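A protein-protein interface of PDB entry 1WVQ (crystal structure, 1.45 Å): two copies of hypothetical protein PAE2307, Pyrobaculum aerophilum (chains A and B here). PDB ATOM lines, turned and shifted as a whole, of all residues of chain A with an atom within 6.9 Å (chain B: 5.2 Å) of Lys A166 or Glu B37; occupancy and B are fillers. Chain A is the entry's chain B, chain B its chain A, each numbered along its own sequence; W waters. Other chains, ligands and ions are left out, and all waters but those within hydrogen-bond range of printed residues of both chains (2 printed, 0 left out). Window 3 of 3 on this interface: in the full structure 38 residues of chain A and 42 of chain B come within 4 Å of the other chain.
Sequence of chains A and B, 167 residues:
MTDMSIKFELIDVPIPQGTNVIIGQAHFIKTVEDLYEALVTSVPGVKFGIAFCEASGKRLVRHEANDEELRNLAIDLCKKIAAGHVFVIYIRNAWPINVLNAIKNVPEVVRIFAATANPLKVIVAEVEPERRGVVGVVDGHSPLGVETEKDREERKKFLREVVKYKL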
ATOM      1  N   LYS A 156     -18.947   7.947  27.827  1.00  0.00           N
ATOM      2  CA  LYS A 156     -18.682   7.908  26.395  1.00  0.00           C
ATOM      3  C   LYS A 156     -18.258   6.506  25.961  1.00  0.00           C
ATOM      4  O   LYS A 156     -18.695   6.014  24.920  1.00  0.00           O
ATOM      5  CB  LYS A 156     -17.592   8.925  26.029  1.00  0.00           C
ATOM      6  CG  LYS A 156     -18.089  10.369  25.941  1.00  0.00           C
ATOM      7  CD  LYS A 156     -16.946  11.389  25.944  1.00  0.00           C
ATOM      8  CE  LYS A 156     -15.862  11.047  24.940  1.00  0.00           C
ATOM      9  NZ  LYS A 156     -14.723  12.013  24.993  1.00  0.00           N
ATOM     10  N   LEU A 159     -21.244   4.048  25.816  1.00  0.00           N
ATOM     11  CA  LEU A 159     -22.054   4.206  24.619  1.00  0.00           C
ATOM     12  C   LEU A 159     -21.366   3.711  23.362  1.00  0.00           C
ATOM     13  O   LEU A 159     -22.022   3.339  22.393  1.00  0.00           O
ATOM     14  CB  LEU A 159     -22.443   5.679  24.442  1.00  0.00           C
ATOM     15  CG  LEU A 159     -23.365   6.268  25.510  1.00  0.00           C
ATOM     16  CD1 LEU A 159     -23.492   7.773  25.306  1.00  0.00           C
ATOM     17  CD2 LEU A 159     -24.728   5.588  25.443  1.00  0.00           C
ATOM     18  N   ARG A 160     -20.040   3.689  23.379  1.00  0.00           N
ATOM     19  CA  ARG A 160     -19.288   3.263  22.210  1.00  0.00           C
ATOM     20  C   ARG A 160     -18.803   1.817  22.208  1.00  0.00           C
ATOM     21  O   ARG A 160     -18.793   1.166  21.165  1.00  0.00           O
ATOM     22  CB  ARG A 160     -18.110   4.223  22.012  1.00  0.00           C
ATOM     23  CG  ARG A 160     -18.578   5.614  21.609  1.00  0.00           C
ATOM     24  CD  ARG A 160     -17.546   6.714  21.831  1.00  0.00           C
ATOM     25  NE  ARG A 160     -18.095   8.001  21.404  1.00  0.00           N
ATOM     26  CZ  ARG A 160     -19.073   8.646  22.035  1.00  0.00           C
ATOM     27  NH1 ARG A 160     -19.609   8.137  23.137  1.00  0.00           N
ATOM     28  NH2 ARG A 160     -19.551   9.777  21.534  1.00  0.00           N
ATOM     29  N   GLU A 161     -18.426   1.304  23.373  1.00  0.00           N
ATOM     30  CA  GLU A 161     -17.919  -0.057  23.462  1.00  0.00           C
ATOM     31  C   GLU A 161     -18.918  -1.108  23.943  1.00  0.00           C
ATOM     32  O   GLU A 161     -18.827  -2.272  23.549  1.00  0.00           O
ATOM     33  CB  GLU A 161     -16.666  -0.063  24.344  1.00  0.00           C
ATOM     34  CG  GLU A 161     -15.480   0.630  23.679  1.00  0.00           C
ATOM     35  CD  GLU A 161     -14.298   0.800  24.611  1.00  0.00           C
ATOM     36  OE1 GLU A 161     -14.098  -0.082  25.467  1.00  0.00           O
ATOM     37  OE2 GLU A 161     -13.560   1.807  24.477  1.00  0.00           O
ATOM     38  N   VAL A 163     -22.910  -0.625  24.405  1.00  0.00           N
ATOM     39  CA  VAL A 163     -24.138  -0.640  23.610  1.00  0.00           C
ATOM     40  C   VAL A 163     -23.882  -0.289  22.146  1.00  0.00           C
ATOM     41  O   VAL A 163     -24.715  -0.541  21.278  1.00  0.00           O
ATOM     42  CB  VAL A 163     -25.219   0.305  24.189  1.00  0.00           C
ATOM     43  CG1 VAL A 163     -25.794  -0.300  25.454  1.00  0.00           C
ATOM     44  CG2 VAL A 163     -24.633   1.682  24.479  1.00  0.00           C
ATOM     45  N   LYS A 164     -22.724   0.302  21.883  1.00  0.00           N
ATOM     46  CA  LYS A 164     -22.326   0.645  20.524  1.00  0.00           C
ATOM     47  C   LYS A 164     -23.305   1.552  19.775  1.00  0.00           C
ATOM     48  O   LYS A 164     -23.485   1.413  18.561  1.00  0.00           O
ATOM     49  CB  LYS A 164     -22.093  -0.646  19.728  1.00  0.00           C
ATOM     50  CG  LYS A 164     -21.126  -1.620  20.414  1.00  0.00           C
ATOM     51  CD  LYS A 164     -20.796  -2.806  19.519  1.00  0.00           C
ATOM     52  CE  LYS A 164     -19.990  -3.852  20.275  1.00  0.00           C
ATOM     53  NZ  LYS A 164     -18.762  -3.289  20.898  1.00  0.00           N
ATOM     54  N   TYR A 165     -23.928   2.483  20.490  1.00  0.00           N
ATOM     55  CA  TYR A 165     -24.868   3.406  19.854  1.00  0.00           C
ATOM     56  C   TYR A 165     -24.159   4.653  19.328  1.00  0.00           C
ATOM     57  O   TYR A 165     -24.759   5.472  18.631  1.00  0.00           O
ATOM     58  CB  TYR A 165     -25.966   3.832  20.831  1.00  0.00           C
ATOM     59  CG  TYR A 165     -26.893   2.720  21.271  1.00  0.00           C
ATOM     60  CD1 TYR A 165     -27.151   1.622  20.448  1.00  0.00           C
ATOM     61  CD2 TYR A 165     -27.561   2.799  22.491  1.00  0.00           C
ATOM     62  CE1 TYR A 165     -28.058   0.634  20.833  1.00  0.00           C
ATOM     63  CE2 TYR A 165     -28.467   1.822  22.883  1.00  0.00           C
ATOM     64  CZ  TYR A 165     -28.713   0.745  22.053  1.00  0.00           C
ATOM     65  OH  TYR A 165     -29.622  -0.211  22.448  1.00  0.00           O
ATOM     66  N   LYS A 166     -22.886   4.797  19.676  1.00  0.00           N
ATOM     67  CA  LYS A 166     -22.082   5.922  19.222  1.00  0.00           C
ATOM     68  C   LYS A 166     -20.745   5.373  18.743  1.00  0.00           C
ATOM     69  O   LYS A 166     -20.369   4.252  19.091  1.00  0.00           O
ATOM     70  CB  LYS A 166     -21.849   6.925  20.357  1.00  0.00           C
ATOM     71  CG  LYS A 166     -23.097   7.683  20.803  1.00  0.00           C
ATOM     72  CD  LYS A 166     -23.654   8.590  19.701  1.00  0.00           C
ATOM     73  CE  LYS A 166     -24.860   9.375  20.216  1.00  0.00           C
ATOM     74  NZ  LYS A 166     -25.514  10.210  19.158  1.00  0.00           N
ATOM     75  N   LEU A 167     -20.033   6.165  17.949  1.00  0.00           N
ATOM     76  CA  LEU A 167     -18.730   5.765  17.431  1.00  0.00           C
ATOM     77  C   LEU A 167     -17.607   6.588  18.072  1.00  0.00           C
ATOM     78  O   LEU A 167     -16.440   6.159  17.973  1.00  0.00           O
ATOM     79  CB  LEU A 167     -18.709   5.920  15.906  1.00  0.00           C
ATOM     80  CG  LEU A 167     -19.755   5.073  15.166  1.00  0.00           C
ATOM     81  CD1 LEU A 167     -19.850   5.510  13.707  1.00  0.00           C
ATOM     82  CD2 LEU A 167     -19.389   3.593  15.276  1.00  0.00           C
ATOM     83  OXT LEU A 167     -17.901   7.652  18.657  1.00  0.00           O
ATOM     84  N   LYS B  30     -27.872   8.203  26.928  1.00  0.00           N
ATOM     85  CA  LYS B  30     -27.540   8.728  25.606  1.00  0.00           C
ATOM     86  C   LYS B  30     -28.215  10.078  25.341  1.00  0.00           C
ATOM     87  O   LYS B  30     -27.827  10.801  24.431  1.00  0.00           O
ATOM     88  CB  LYS B  30     -27.922   7.713  24.524  1.00  0.00           C
ATOM     89  CG  LYS B  30     -27.321   8.015  23.147  1.00  0.00           C
ATOM     90  CD  LYS B  30     -27.341   6.787  22.231  1.00  0.00           C
ATOM     91  CE  LYS B  30     -28.741   6.416  21.749  1.00  0.00           C
ATOM     92  NZ  LYS B  30     -29.216   7.338  20.674  1.00  0.00           N
ATOM     93  N   GLU B  33     -25.864  13.153  24.882  1.00  0.00           N
ATOM     94  CA  GLU B  33     -25.153  13.268  23.614  1.00  0.00           C
ATOM     95  C   GLU B  33     -26.100  13.599  22.466  1.00  0.00           C
ATOM     96  O   GLU B  33     -25.772  14.412  21.598  1.00  0.00           O
ATOM     97  CB  GLU B  33     -24.383  11.980  23.311  1.00  0.00           C
ATOM     98  CG  GLU B  33     -23.262  11.722  24.314  1.00  0.00           C
ATOM     99  CD  GLU B  33     -22.167  10.807  23.785  1.00  0.00           C
ATOM    100  OE1 GLU B  33     -22.032  10.666  22.551  1.00  0.00           O
ATOM    101  OE2 GLU B  33     -21.425  10.252  24.618  1.00  0.00           O
ATOM    102  N   ASP B  34     -27.279  12.991  22.455  1.00  0.00           N
ATOM    103  CA  ASP B  34     -28.220  13.267  21.379  1.00  0.00           C
ATOM    104  C   ASP B  34     -28.707  14.713  21.401  1.00  0.00           C
ATOM    105  O   ASP B  34     -28.897  15.321  20.346  1.00  0.00           O
ATOM    106  CB  ASP B  34     -29.404  12.296  21.433  1.00  0.00           C
ATOM    107  CG  ASP B  34     -29.011  10.871  21.044  1.00  0.00           C
ATOM    108  OD1 ASP B  34     -27.912  10.672  20.475  1.00  0.00           O
ATOM    109  OD2 ASP B  34     -29.815   9.946  21.290  1.00  0.00           O
ATOM    110  N   LEU B  35     -28.899  15.273  22.592  1.00  0.00           N
ATOM    111  CA  LEU B  35     -29.331  16.662  22.692  1.00  0.00           C
ATOM    112  C   LEU B  35     -28.189  17.588  22.266  1.00  0.00           C
ATOM    113  O   LEU B  35     -28.417  18.600  21.610  1.00  0.00           O
ATOM    114  CB  LEU B  35     -29.796  16.984  24.119  1.00  0.00           C
ATOM    115  CG  LEU B  35     -31.161  16.402  24.515  1.00  0.00           C
ATOM    116  CD1 LEU B  35     -31.471  16.768  25.955  1.00  0.00           C
ATOM    117  CD2 LEU B  35     -32.248  16.944  23.587  1.00  0.00           C
ATOM    118  N   TYR B  36     -26.960  17.238  22.630  1.00  0.00           N
ATOM    119  CA  TYR B  36     -25.812  18.044  22.233  1.00  0.00           C
ATOM    120  C   TYR B  36     -25.786  18.124  20.705  1.00  0.00           C
ATOM    121  O   TYR B  36     -25.615  19.195  20.126  1.00  0.00           O
ATOM    122  CB  TYR B  36     -24.510  17.406  22.749  1.00  0.00           C
ATOM    123  CG  TYR B  36     -23.253  17.955  22.097  1.00  0.00           C
ATOM    124  CD1 TYR B  36     -22.789  17.443  20.887  1.00  0.00           C
ATOM    125  CD2 TYR B  36     -22.560  19.019  22.667  1.00  0.00           C
ATOM    126  CE1 TYR B  36     -21.669  17.981  20.256  1.00  0.00           C
ATOM    127  CE2 TYR B  36     -21.439  19.563  22.048  1.00  0.00           C
ATOM    128  CZ  TYR B  36     -21.003  19.044  20.845  1.00  0.00           C
ATOM    129  OH  TYR B  36     -19.919  19.609  20.218  1.00  0.00           O
ATOM    130  N   GLU B  37     -25.969  16.979  20.060  1.00  0.00           N
ATOM    131  CA  GLU B  37     -25.947  16.912  18.604  1.00  0.00           C
ATOM    132  C   GLU B  37     -27.087  17.679  17.957  1.00  0.00           C
ATOM    133  O   GLU B  37     -26.891  18.368  16.957  1.00  0.00           O
ATOM    134  CB  GLU B  37     -25.954  15.449  18.158  1.00  0.00           C
ATOM    135  CG  GLU B  37     -24.635  14.745  18.452  1.00  0.00           C
ATOM    136  CD  GLU B  37     -24.576  13.339  17.902  1.00  0.00           C
ATOM    137  OE1 GLU B  37     -25.085  13.114  16.790  1.00  0.00           O
ATOM    138  OE2 GLU B  37     -24.001  12.462  18.575  1.00  0.00           O
ATOM    139  N   ALA B  38     -28.278  17.569  18.532  1.00  0.00           N
ATOM    140  CA  ALA B  38     -29.439  18.267  17.998  1.00  0.00           C
ATOM    141  C   ALA B  38     -29.184  19.773  17.984  1.00  0.00           C
ATOM    142  O   ALA B  38     -29.561  20.472  17.043  1.00  0.00           O
ATOM    143  CB  ALA B  38     -30.666  17.948  18.847  1.00  0.00           C
ATOM    144  N   LEU B  39     -28.529  20.266  19.030  1.00  0.00           N
ATOM    145  CA  LEU B  39     -28.242  21.689  19.129  1.00  0.00           C
ATOM    146  C   LEU B  39     -27.138  22.160  18.184  1.00  0.00           C
ATOM    147  O   LEU B  39     -27.352  23.079  17.395  1.00  0.00           O
ATOM    148  CB  LEU B  39     -27.886  22.049  20.577  1.00  0.00           C
ATOM    149  CG  LEU B  39     -29.016  21.832  21.591  1.00  0.00           C
ATOM    150  CD1 LEU B  39     -28.461  21.919  23.002  1.00  0.00           C
ATOM    151  CD2 LEU B  39     -30.116  22.864  21.388  1.00  0.00           C
ATOM    152  N   VAL B  40     -25.970  21.522  18.239  1.00  0.00           N
ATOM    153  CA  VAL B  40     -24.852  21.940  17.394  1.00  0.00           C
ATOM    154  C   VAL B  40     -25.084  21.814  15.893  1.00  0.00           C
ATOM    155  O   VAL B  40     -24.488  22.556  15.114  1.00  0.00           O
ATOM    156  CB  VAL B  40     -23.534  21.184  17.750  1.00  0.00           C
ATOM    157  CG1 VAL B  40     -23.220  21.349  19.217  1.00  0.00           C
ATOM    158  CG2 VAL B  40     -23.632  19.708  17.377  1.00  0.00           C
ATOM    159  N   THR B  41     -25.949  20.891  15.480  1.00  0.00           N
ATOM    160  CA  THR B  41     -26.217  20.702  14.056  1.00  0.00           C
ATOM    161  C   THR B  41     -27.403  21.527  13.563  1.00  0.00           C
ATOM    162  O   THR B  41     -27.737  21.495  12.378  1.00  0.00           O
ATOM    163  CB  THR B  41     -26.479  19.210  13.722  1.00  0.00           C
ATOM    164  OG1 THR B  41     -27.627  18.744  14.441  1.00  0.00           O
ATOM    165  CG2 THR B  41     -25.276  18.364  14.095  1.00  0.00           C
ATOM    166  N   SER B  42     -28.029  22.271  14.467  1.00  0.00           N
ATOM    167  CA  SER B  42     -29.178  23.092  14.103  1.00  0.00           C
ATOM    168  C   SER B  42     -28.817  24.509  13.683  1.00  0.00           C
ATOM    169  O   SER B  42     -29.393  25.028  12.734  1.00  0.00           O
ATOM    170  CB  SER B  42     -30.176  23.183  15.262  1.00  0.00           C
ATOM    171  OG  SER B  42     -30.928  21.992  15.397  1.00  0.00           O
HETATM  172  O   HOH W   1     -27.062   6.974  18.717  1.00  0.00           O
HETATM  173  O   HOH W   2     -21.710  11.930  19.978  1.00  0.00           O
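OE1 of Glu B33 lies within salt-bridge range of NH2 of Arg A160 (2.8 Å). The side-chain carboxylate of Asp B34 is in salt-bridge range of the side-chain amino group of Lys A166. The side-chain amino group (NZ) of Lys A166 lies within salt-bridge range of the side-chain carboxylate (OE2) of Glu B37 (2.8 Å).
Among the printed residues, merely in contact across the chains: Leu A159 with Glu B33 (3.3 Å), Tyr A165 with Lys B30 (3.5 Å), Lys A156 with Glu B33 (3.6 Å), Lys A166 with Glu B33 (3.6 Å) and Leu A159 with Lys B30 (3.9 Å).
Of the 11 printed residues of chain B, 4 touch a printed residue of chain A. Of the 9 printed residues of chain A, 5 touch a printed residue of chain B. Printed residues of chain A that touch a printed residue of chain B: Lys A156, Leu A159, Arg A160, Tyr A165 and Lys A166. Hydrophobic or aromatic side chains of chain A within 4 Å of the printed part of chain B: Leu A159 and Tyr A165. Along chain A the printed residues that touch a printed residue of chain B span positions 156 to 166. Among the printed residues, 8 pairs touch across the chains. Among the printed residues, Asp or Glu carboxylates within 4 Å of a Lys or Arg side-chain nitrogen of the other chain: Arg A160 with Glu B33 (2.8 Å), Lys A166 with Asp B34 (2.8 Å) and Lys A166 with Glu B37 (2.8 Å).
OG1 of Thr B41 is in hydrogen-bond range of O of Glu B37 (2.6 Å). O of Lys A156 lies within hydrogen-bond range of NH1 of Arg A160 (2.9 Å). O of Leu A159 is in hydrogen-bond range of N of Lys A164, 3.2 Å away. The backbone carbonyl oxygen (O) of Leu A159 sits at hydrogen-bond distance from the backbone NH (N) of Tyr A165 (2.8 Å). The backbone carbonyl oxygen (O) of Leu A159 is in hydrogen-bond range of the backbone NH (N) of Lys A166 (3.2 Å). The guanidinium group (NE) of Arg A160 lies within salt-bridge range of the chain-end carboxylate (OXT) of Leu A167 (2.8 Å).
Water W2 lies within hydrogen-bond range of OE2 of Glu B37, OE1 of Glu B33 and NH2 of Arg A160. Water W1 lies within hydrogen-bond range of O of Tyr A165 (2.8 Å) and NZ of Lys B30 (2.9 Å).
No position is printed for both chains. Of the 8 pairs that touch across the chains among the printed residues, none has its exchanged pair printed and touching as well.
Of the printed residues of chain B, Tyr A165 touches Lys B30 (3.5 Å). Lys A166 touches just these residues of chain B: Glu B33 (3.6 Å), Asp B34 (2.8 Å) and Glu B37 (2.8 Å). Of the printed residues of chain A, Lys B30 touches Leu A159 and Tyr A165. Of the printed residues of chain A, Asp B34 touches Lys A166. Val B40 touches none of the printed residues of chain A. Thr B41 touches none of the printed residues of chain A. The nearest residue of chain B that does not touch Lys A166 is Lys B30 (4.1 Å). The nearest residue of chain A that does not touch Glu B37 is Arg A160 (6.0 Å).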
